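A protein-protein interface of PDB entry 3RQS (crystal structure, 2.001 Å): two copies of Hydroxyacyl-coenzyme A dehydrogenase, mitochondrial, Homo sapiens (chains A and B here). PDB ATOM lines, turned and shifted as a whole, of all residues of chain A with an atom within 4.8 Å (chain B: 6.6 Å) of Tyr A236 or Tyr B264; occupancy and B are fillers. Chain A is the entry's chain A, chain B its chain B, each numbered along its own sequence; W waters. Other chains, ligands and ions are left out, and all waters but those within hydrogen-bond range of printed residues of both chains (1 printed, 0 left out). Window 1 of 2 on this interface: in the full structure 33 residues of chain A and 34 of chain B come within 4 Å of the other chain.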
ATOM      1  N   LEU A 232     -16.026 -21.737  -6.286  1.00  0.00           N
ATOM      2  CA  LEU A 232     -16.915 -21.743  -7.440  1.00  0.00           C
ATOM      3  C   LEU A 232     -17.937 -20.622  -7.355  1.00  0.00           C
ATOM      4  O   LEU A 232     -18.425 -20.133  -8.373  1.00  0.00           O
ATOM      5  CB  LEU A 232     -17.616 -23.095  -7.563  1.00  0.00           C
ATOM      6  CG  LEU A 232     -16.623 -24.245  -7.766  1.00  0.00           C
ATOM      7  CD1 LEU A 232     -17.332 -25.596  -7.841  1.00  0.00           C
ATOM      8  CD2 LEU A 232     -15.810 -24.002  -9.027  1.00  0.00           C
ATOM      9  N   LEU A 233     -18.250 -20.207  -6.135  1.00  0.00           N
ATOM     10  CA  LEU A 233     -19.257 -19.178  -5.921  1.00  0.00           C
ATOM     11  C   LEU A 233     -18.677 -17.775  -6.086  1.00  0.00           C
ATOM     12  O   LEU A 233     -19.203 -16.950  -6.823  1.00  0.00           O
ATOM     13  CB  LEU A 233     -19.849 -19.313  -4.513  1.00  0.00           C
ATOM     14  CG  LEU A 233     -20.890 -18.251  -4.126  1.00  0.00           C
ATOM     15  CD1 LEU A 233     -22.139 -18.404  -4.967  1.00  0.00           C
ATOM     16  CD2 LEU A 233     -21.235 -18.360  -2.667  1.00  0.00           C
ATOM     17  N   VAL A 234     -17.591 -17.498  -5.377  1.00  0.00           N
ATOM     18  CA  VAL A 234     -17.113 -16.122  -5.307  1.00  0.00           C
ATOM     19  C   VAL A 234     -16.685 -15.563  -6.673  1.00  0.00           C
ATOM     20  O   VAL A 234     -17.039 -14.432  -7.014  1.00  0.00           O
ATOM     21  CB  VAL A 234     -16.054 -15.949  -4.205  1.00  0.00           C
ATOM     22  CG1 VAL A 234     -15.450 -14.535  -4.234  1.00  0.00           C
ATOM     23  CG2 VAL A 234     -16.696 -16.221  -2.858  1.00  0.00           C
ATOM     24  N   PRO A 235     -15.954 -16.358  -7.476  1.00  0.00           N
ATOM     25  CA  PRO A 235     -15.593 -15.832  -8.797  1.00  0.00           C
ATOM     26  C   PRO A 235     -16.814 -15.567  -9.680  1.00  0.00           C
ATOM     27  O   PRO A 235     -16.777 -14.645 -10.497  1.00  0.00           O
ATOM     28  CB  PRO A 235     -14.716 -16.941  -9.386  1.00  0.00           C
ATOM     29  CG  PRO A 235     -14.074 -17.565  -8.160  1.00  0.00           C
ATOM     30  CD  PRO A 235     -15.189 -17.575  -7.140  1.00  0.00           C
ATOM     31  N   TYR A 236     -17.870 -16.358  -9.524  1.00  0.00           N
ATOM     32  CA  TYR A 236     -19.124 -16.094 -10.229  1.00  0.00           C
ATOM     33  C   TYR A 236     -19.736 -14.756  -9.801  1.00  0.00           C
ATOM     34  O   TYR A 236     -20.171 -13.967 -10.637  1.00  0.00           O
ATOM     35  CB  TYR A 236     -20.114 -17.255 -10.017  1.00  0.00           C
ATOM     36  CG  TYR A 236     -21.555 -16.838  -9.916  1.00  0.00           C
ATOM     37  CD1 TYR A 236     -22.222 -16.310 -11.016  1.00  0.00           C
ATOM     38  CD2 TYR A 236     -22.259 -16.977  -8.719  1.00  0.00           C
ATOM     39  CE1 TYR A 236     -23.541 -15.918 -10.933  1.00  0.00           C
ATOM     40  CE2 TYR A 236     -23.592 -16.593  -8.623  1.00  0.00           C
ATOM     41  CZ  TYR A 236     -24.224 -16.070  -9.735  1.00  0.00           C
ATOM     42  OH  TYR A 236     -25.532 -15.681  -9.658  1.00  0.00           O
ATOM     43  N   LEU A 237     -19.784 -14.509  -8.496  1.00  0.00           N
ATOM     44  CA  LEU A 237     -20.276 -13.235  -7.997  1.00  0.00           C
ATOM     45  C   LEU A 237     -19.475 -12.074  -8.580  1.00  0.00           C
ATOM     46  O   LEU A 237     -20.046 -11.052  -8.955  1.00  0.00           O
ATOM     47  CB  LEU A 237     -20.208 -13.190  -6.466  1.00  0.00           C
ATOM     48  CG  LEU A 237     -21.062 -14.242  -5.757  1.00  0.00           C
ATOM     49  CD1 LEU A 237     -20.870 -14.123  -4.268  1.00  0.00           C
ATOM     50  CD2 LEU A 237     -22.540 -14.100  -6.160  1.00  0.00           C
ATOM     51  N   MET A 238     -18.152 -12.229  -8.639  1.00  0.00           N
ATOM     52  CA  MET A 238     -17.303 -11.181  -9.186  1.00  0.00           C
ATOM     53  C   MET A 238     -17.648 -10.969 -10.655  1.00  0.00           C
ATOM     54  O   MET A 238     -17.659  -9.838 -11.137  1.00  0.00           O
ATOM     55  CB  MET A 238     -15.818 -11.539  -9.042  1.00  0.00           C
ATOM     56  CG  MET A 238     -15.310 -11.579  -7.605  1.00  0.00           C
ATOM     57  SD  MET A 238     -15.625  -9.860  -6.699  1.00  0.00           S
ATOM     58  CE  MET A 238     -14.470  -8.741  -7.811  1.00  0.00           C
ATOM     59  N   GLU A 239     -17.913 -12.061 -11.372  1.00  0.00           N
ATOM     60  CA  GLU A 239     -18.275 -11.967 -12.787  1.00  0.00           C
ATOM     61  C   GLU A 239     -19.623 -11.255 -12.971  1.00  0.00           C
ATOM     62  O   GLU A 239     -19.796 -10.496 -13.922  1.00  0.00           O
ATOM     63  CB  GLU A 239     -18.287 -13.353 -13.455  1.00  0.00           C
ATOM     64  CG  GLU A 239     -16.873 -13.832 -13.877  1.00  0.00           C
ATOM     65  CD  GLU A 239     -16.291 -13.003 -15.024  1.00  0.00           C
ATOM     66  OE1 GLU A 239     -16.506 -13.353 -16.200  1.00  0.00           O
ATOM     67  OE2 GLU A 239     -15.633 -11.986 -14.761  1.00  0.00           O
ATOM     68  N   ALA A 240     -20.566 -11.493 -12.061  1.00  0.00           N
ATOM     69  CA  ALA A 240     -21.838 -10.774 -12.123  1.00  0.00           C
ATOM     70  C   ALA A 240     -21.563  -9.270 -11.959  1.00  0.00           C
ATOM     71  O   ALA A 240     -22.078  -8.452 -12.705  1.00  0.00           O
ATOM     72  CB  ALA A 240     -22.788 -11.264 -11.038  1.00  0.00           C
ATOM     73  N   MET A 258     -30.632 -14.970 -12.982  1.00  0.00           N
ATOM     74  CA  MET A 258     -30.074 -16.110 -12.277  1.00  0.00           C
ATOM     75  C   MET A 258     -31.141 -16.849 -11.460  1.00  0.00           C
ATOM     76  O   MET A 258     -31.118 -18.079 -11.384  1.00  0.00           O
ATOM     77  CB  MET A 258     -28.903 -15.686 -11.386  1.00  0.00           C
ATOM     78  CG  MET A 258     -27.775 -15.009 -12.141  1.00  0.00           C
ATOM     79  SD  MET A 258     -27.332 -15.930 -13.836  1.00  0.00           S
ATOM     80  CE  MET A 258     -26.513 -17.569 -13.140  1.00  0.00           C
ATOM     81  N   TYR A 264     -31.415 -20.015  -8.908  1.00  0.00           N
ATOM     82  CA  TYR A 264     -30.657 -19.652  -7.716  1.00  0.00           C
ATOM     83  C   TYR A 264     -31.574 -19.012  -6.689  1.00  0.00           C
ATOM     84  O   TYR A 264     -32.459 -18.258  -7.047  1.00  0.00           O
ATOM     85  CB  TYR A 264     -29.538 -18.679  -8.060  1.00  0.00           C
ATOM     86  CG  TYR A 264     -28.418 -19.308  -8.846  1.00  0.00           C
ATOM     87  CD1 TYR A 264     -28.479 -20.644  -9.225  1.00  0.00           C
ATOM     88  CD2 TYR A 264     -27.284 -18.573  -9.186  1.00  0.00           C
ATOM     89  CE1 TYR A 264     -27.442 -21.233  -9.947  1.00  0.00           C
ATOM     90  CE2 TYR A 264     -26.256 -19.144  -9.906  1.00  0.00           C
ATOM     91  CZ  TYR A 264     -26.336 -20.481 -10.279  1.00  0.00           C
ATOM     92  OH  TYR A 264     -25.309 -21.068 -10.991  1.00  0.00           O
ATOM     93  N   PRO A 265     -31.363 -19.317  -5.406  1.00  0.00           N
ATOM     94  CA  PRO A 265     -32.219 -18.758  -4.355  1.00  0.00           C
ATOM     95  C   PRO A 265     -32.096 -17.241  -4.321  1.00  0.00           C
ATOM     96  O   PRO A 265     -33.069 -16.529  -4.081  1.00  0.00           O
ATOM     97  CB  PRO A 265     -31.619 -19.339  -3.073  1.00  0.00           C
ATOM     98  CG  PRO A 265     -30.848 -20.536  -3.501  1.00  0.00           C
ATOM     99  CD  PRO A 265     -30.355 -20.250  -4.879  1.00  0.00           C
ATOM    100  N   GLY A 267     -30.248 -13.791  -6.423  1.00  0.00           N
ATOM    101  CA  GLY A 267     -29.453 -13.176  -7.465  1.00  0.00           C
ATOM    102  C   GLY A 267     -28.082 -12.846  -6.919  1.00  0.00           C
ATOM    103  O   GLY A 267     -27.901 -12.729  -5.710  1.00  0.00           O
ATOM    104  N   PRO A 268     -27.093 -12.698  -7.802  1.00  0.00           N
ATOM    105  CA  PRO A 268     -25.743 -12.530  -7.254  1.00  0.00           C
ATOM    106  C   PRO A 268     -25.586 -11.229  -6.452  1.00  0.00           C
ATOM    107  O   PRO A 268     -24.799 -11.183  -5.513  1.00  0.00           O
ATOM    108  CB  PRO A 268     -24.854 -12.497  -8.503  1.00  0.00           C
ATOM    109  CG  PRO A 268     -25.786 -12.139  -9.643  1.00  0.00           C
ATOM    110  CD  PRO A 268     -27.107 -12.769  -9.271  1.00  0.00           C
ATOM    111  N   LEU B 232     -22.767 -16.177 -17.041  1.00  0.00           N
ATOM    112  CA  LEU B 232     -22.452 -16.347 -15.637  1.00  0.00           C
ATOM    113  C   LEU B 232     -22.499 -17.806 -15.211  1.00  0.00           C
ATOM    114  O   LEU B 232     -21.773 -18.218 -14.312  1.00  0.00           O
ATOM    115  CB  LEU B 232     -23.411 -15.520 -14.774  1.00  0.00           C
ATOM    116  CG  LEU B 232     -23.276 -14.017 -15.022  1.00  0.00           C
ATOM    117  CD1 LEU B 232     -24.255 -13.229 -14.154  1.00  0.00           C
ATOM    118  CD2 LEU B 232     -21.843 -13.560 -14.781  1.00  0.00           C
ATOM    119  N   LEU B 233     -23.348 -18.586 -15.870  1.00  0.00           N
ATOM    120  CA  LEU B 233     -23.518 -19.993 -15.521  1.00  0.00           C
ATOM    121  C   LEU B 233     -22.414 -20.874 -16.117  1.00  0.00           C
ATOM    122  O   LEU B 233     -21.796 -21.676 -15.428  1.00  0.00           O
ATOM    123  CB  LEU B 233     -24.883 -20.493 -16.025  1.00  0.00           C
ATOM    124  CG  LEU B 233     -25.177 -21.983 -15.855  1.00  0.00           C
ATOM    125  CD1 LEU B 233     -25.269 -22.304 -14.380  1.00  0.00           C
ATOM    126  CD2 LEU B 233     -26.487 -22.388 -16.586  1.00  0.00           C
ATOM    127  N   TYR B 236     -18.923 -20.931 -14.775  1.00  0.00           N
ATOM    128  CA  TYR B 236     -18.919 -21.534 -13.448  1.00  0.00           C
ATOM    129  C   TYR B 236     -18.918 -23.060 -13.572  1.00  0.00           C
ATOM    130  O   TYR B 236     -18.180 -23.756 -12.871  1.00  0.00           O
ATOM    131  CB  TYR B 236     -20.116 -21.037 -12.623  1.00  0.00           C
ATOM    132  CG  TYR B 236     -20.747 -22.098 -11.754  1.00  0.00           C
ATOM    133  CD1 TYR B 236     -20.096 -22.582 -10.623  1.00  0.00           C
ATOM    134  CD2 TYR B 236     -21.994 -22.614 -12.060  1.00  0.00           C
ATOM    135  CE1 TYR B 236     -20.674 -23.563  -9.824  1.00  0.00           C
ATOM    136  CE2 TYR B 236     -22.583 -23.591 -11.270  1.00  0.00           C
ATOM    137  CZ  TYR B 236     -21.914 -24.059 -10.148  1.00  0.00           C
ATOM    138  OH  TYR B 236     -22.486 -25.030  -9.368  1.00  0.00           O
ATOM    139  N   ASP B 255     -20.967 -31.362  -6.280  1.00  0.00           N
ATOM    140  CA  ASP B 255     -22.416 -31.245  -6.435  1.00  0.00           C
ATOM    141  C   ASP B 255     -23.107 -31.024  -5.088  1.00  0.00           C
ATOM    142  O   ASP B 255     -23.949 -30.136  -4.948  1.00  0.00           O
ATOM    143  CB  ASP B 255     -22.996 -32.460  -7.156  1.00  0.00           C
ATOM    144  CG  ASP B 255     -22.737 -32.424  -8.667  1.00  0.00           C
ATOM    145  OD1 ASP B 255     -22.147 -31.437  -9.153  1.00  0.00           O
ATOM    146  OD2 ASP B 255     -23.106 -33.388  -9.368  1.00  0.00           O
ATOM    147  N   MET B 258     -22.395 -27.471  -3.782  1.00  0.00           N
ATOM    148  CA  MET B 258     -23.162 -26.384  -4.387  1.00  0.00           C
ATOM    149  C   MET B 258     -24.659 -26.456  -4.043  1.00  0.00           C
ATOM    150  O   MET B 258     -25.317 -25.432  -3.913  1.00  0.00           O
ATOM    151  CB  MET B 258     -22.937 -26.328  -5.897  1.00  0.00           C
ATOM    152  CG  MET B 258     -21.467 -26.149  -6.294  1.00  0.00           C
ATOM    153  SD  MET B 258     -20.538 -24.733  -5.276  1.00  0.00           S
ATOM    154  CE  MET B 258     -19.754 -25.826  -3.897  1.00  0.00           C
ATOM    155  N   LYS B 259     -25.199 -27.660  -3.890  1.00  0.00           N
ATOM    156  CA  LYS B 259     -26.602 -27.775  -3.509  1.00  0.00           C
ATOM    157  C   LYS B 259     -26.803 -27.303  -2.068  1.00  0.00           C
ATOM    158  O   LYS B 259     -27.690 -26.502  -1.785  1.00  0.00           O
ATOM    159  CB  LYS B 259     -27.115 -29.210  -3.687  1.00  0.00           C
ATOM    160  CG  LYS B 259     -27.340 -29.601  -5.159  1.00  0.00           C
ATOM    161  CD  LYS B 259     -28.041 -30.968  -5.295  1.00  0.00           C
ATOM    162  CE  LYS B 259     -27.143 -32.114  -4.868  1.00  0.00           C
ATOM    163  NZ  LYS B 259     -27.813 -33.442  -5.028  1.00  0.00           N
ATOM    164  N   LEU B 260     -25.963 -27.795  -1.167  1.00  0.00           N
ATOM    165  CA  LEU B 260     -26.119 -27.504   0.251  1.00  0.00           C
ATOM    166  C   LEU B 260     -25.452 -26.192   0.646  1.00  0.00           C
ATOM    167  O   LEU B 260     -25.910 -25.501   1.549  1.00  0.00           O
ATOM    168  CB  LEU B 260     -25.574 -28.648   1.097  1.00  0.00           C
ATOM    169  CG  LEU B 260     -26.180 -30.030   0.875  1.00  0.00           C
ATOM    170  CD1 LEU B 260     -25.537 -31.045   1.814  1.00  0.00           C
ATOM    171  CD2 LEU B 260     -27.679 -29.996   1.083  1.00  0.00           C
ATOM    172  N   GLY B 261     -24.368 -25.851  -0.038  1.00  0.00           N
ATOM    173  CA  GLY B 261     -23.600 -24.666   0.299  1.00  0.00           C
ATOM    174  C   GLY B 261     -24.132 -23.437  -0.398  1.00  0.00           C
ATOM    175  O   GLY B 261     -24.075 -22.345   0.149  1.00  0.00           O
ATOM    176  N   ALA B 262     -24.663 -23.610  -1.605  1.00  0.00           N
ATOM    177  CA  ALA B 262     -25.110 -22.463  -2.385  1.00  0.00           C
ATOM    178  C   ALA B 262     -26.598 -22.512  -2.690  1.00  0.00           C
ATOM    179  O   ALA B 262     -27.117 -21.604  -3.323  1.00  0.00           O
ATOM    180  CB  ALA B 262     -24.307 -22.347  -3.670  1.00  0.00           C
ATOM    181  N   GLY B 263     -27.274 -23.575  -2.248  1.00  0.00           N
ATOM    182  CA  GLY B 263     -28.710 -23.693  -2.437  1.00  0.00           C
ATOM    183  C   GLY B 263     -29.131 -23.952  -3.878  1.00  0.00           C
ATOM    184  O   GLY B 263     -30.284 -23.730  -4.247  1.00  0.00           O
ATOM    185  N   TYR B 264     -28.198 -24.430  -4.697  1.00  0.00           N
ATOM    186  CA  TYR B 264     -28.500 -24.697  -6.097  1.00  0.00           C
ATOM    187  C   TYR B 264     -29.361 -25.945  -6.220  1.00  0.00           C
ATOM    188  O   TYR B 264     -29.110 -26.938  -5.547  1.00  0.00           O
ATOM    189  CB  TYR B 264     -27.207 -24.882  -6.899  1.00  0.00           C
ATOM    190  CG  TYR B 264     -26.385 -23.617  -7.047  1.00  0.00           C
ATOM    191  CD1 TYR B 264     -26.856 -22.396  -6.580  1.00  0.00           C
ATOM    192  CD2 TYR B 264     -25.137 -23.652  -7.661  1.00  0.00           C
ATOM    193  CE1 TYR B 264     -26.097 -21.229  -6.719  1.00  0.00           C
ATOM    194  CE2 TYR B 264     -24.378 -22.505  -7.813  1.00  0.00           C
ATOM    195  CZ  TYR B 264     -24.859 -21.300  -7.347  1.00  0.00           C
ATOM    196  OH  TYR B 264     -24.089 -20.179  -7.499  1.00  0.00           O
ATOM    197  N   PRO B 265     -30.364 -25.911  -7.104  1.00  0.00           N
ATOM    198  CA  PRO B 265     -31.218 -27.094  -7.268  1.00  0.00           C
ATOM    199  C   PRO B 265     -30.394 -28.308  -7.697  1.00  0.00           C
ATOM    200  O   PRO B 265     -30.667 -29.428  -7.290  1.00  0.00           O
ATOM    201  CB  PRO B 265     -32.160 -26.691  -8.407  1.00  0.00           C
ATOM    202  CG  PRO B 265     -32.168 -25.211  -8.397  1.00  0.00           C
ATOM    203  CD  PRO B 265     -30.800 -24.783  -7.940  1.00  0.00           C
ATOM    204  N   MET B 266     -29.391 -28.076  -8.532  1.00  0.00           N
ATOM    205  CA  MET B 266     -28.534 -29.161  -8.996  1.00  0.00           C
ATOM    206  C   MET B 266     -27.075 -28.737  -8.907  1.00  0.00           C
ATOM    207  O   MET B 266     -26.740 -27.586  -9.185  1.00  0.00           O
ATOM    208  CB  MET B 266     -28.879 -29.536 -10.443  1.00  0.00           C
ATOM    209  CG  MET B 266     -30.176 -30.362 -10.584  1.00  0.00           C
ATOM    210  SD  MET B 266     -30.571 -30.707 -12.493  1.00  0.00           S
ATOM    211  CE  MET B 266     -31.417 -29.014 -12.939  1.00  0.00           C
ATOM    212  N   GLY B 267     -26.216 -29.668  -8.513  1.00  0.00           N
ATOM    213  CA  GLY B 267     -24.793 -29.410  -8.496  1.00  0.00           C
ATOM    214  C   GLY B 267     -24.330 -29.339  -9.934  1.00  0.00           C
ATOM    215  O   GLY B 267     -25.039 -29.796 -10.831  1.00  0.00           O
ATOM    216  N   PRO B 268     -23.137 -28.770 -10.161  1.00  0.00           N
ATOM    217  CA  PRO B 268     -22.716 -28.425 -11.525  1.00  0.00           C
ATOM    218  C   PRO B 268     -22.565 -29.629 -12.436  1.00  0.00           C
ATOM    219  O   PRO B 268     -22.811 -29.491 -13.620  1.00  0.00           O
ATOM    220  CB  PRO B 268     -21.366 -27.722 -11.328  1.00  0.00           C
ATOM    221  CG  PRO B 268     -20.920 -28.094  -9.929  1.00  0.00           C
ATOM    222  CD  PRO B 268     -22.183 -28.294  -9.138  1.00  0.00           C
HETATM  223  O   HOH W   1     -23.231 -19.483 -11.501  1.00  0.00           O
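Water W1 lies within hydrogen-bond range of the side-chain hydroxyl (OH) of Tyr A264 (2.7 Å) and the backbone carbonyl oxygen (O) of Leu B232 (3.4 Å).
The backbone carbonyl oxygen of Met B258 sits at hydrogen-bond distance from the backbone NH of Tyr B264, 3.1 Å away. The backbone carbonyl oxygen of Met A258 lies within hydrogen-bond range of the backbone NH of Tyr A264 (3.2 Å). O of Met B258 lies within hydrogen-bond range of N of Gly B263, at 3.2 Å.
Tyr A236 touches just these residues of chain B: Leu B232 (3.8 Å) and Tyr B264 (3.8 Å). Of chain A, only Leu A233, Tyr A236 and Tyr A264 come within 4 Å of Tyr B264. Printed residues of chain A within 4 Å of Gly B263: Pro A265 (3.3 Å). Of the printed residues of chain B, Tyr A264 touches Leu B233 (3.6 Å), Tyr B236 (3.7 Å) and Tyr B264 (3.4 Å). Printed residues of chain B within 4 Å of Glu A239: Leu B232. Printed residues of chain A within 4 Å of Leu B232: Tyr A236, Glu A239 and Ala A240. Of the printed residues of chain A, Ala B262 touches Pro A265 (3.8 Å). Leu A237 touches none of the printed residues of chain B. The nearest residue of chain B that does not touch Tyr A236 is Tyr B236 (4.6 Å).
Hydrophobic or aromatic side chains of chain B that line the printed part of chain A: Leu B232, Leu B233, Tyr B236 and Tyr B264. Of the 14 printed residues of chain A, 7 touch a printed residue of chain B. Among the printed residues, 11 pairs touch across the chains.
Leu A232 touches Tyr B236, and with the chains exchanged Tyr A236 touches Leu B232. Leu A233 touches Tyr B264, and with the chains exchanged Tyr A264 touches Leu B233. Tyr A236 touches Tyr B264, and with the chains exchanged Tyr A264 touches Tyr B236. Tyr A264 touches its own counterpart, Tyr B264. 8 positions are printed for both chains. Of the 11 pairs that touch across the chains among the printed residues, 7 have their exchanged pair printed and touching as well.
Among the printed residues, merely in contact across the chains: Leu A232 with Tyr B236, Leu A233 with Tyr B264, Tyr A236 with Leu B232, Tyr A236 with Tyr B264, Glu A239 with Leu B232, Ala A240 with Leu B232, Tyr A264 with Leu B233, Tyr A264 with Tyr B236, Tyr A264 with Tyr B264, Pro A265 with Ala B262 and Pro A265 with Gly B263.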
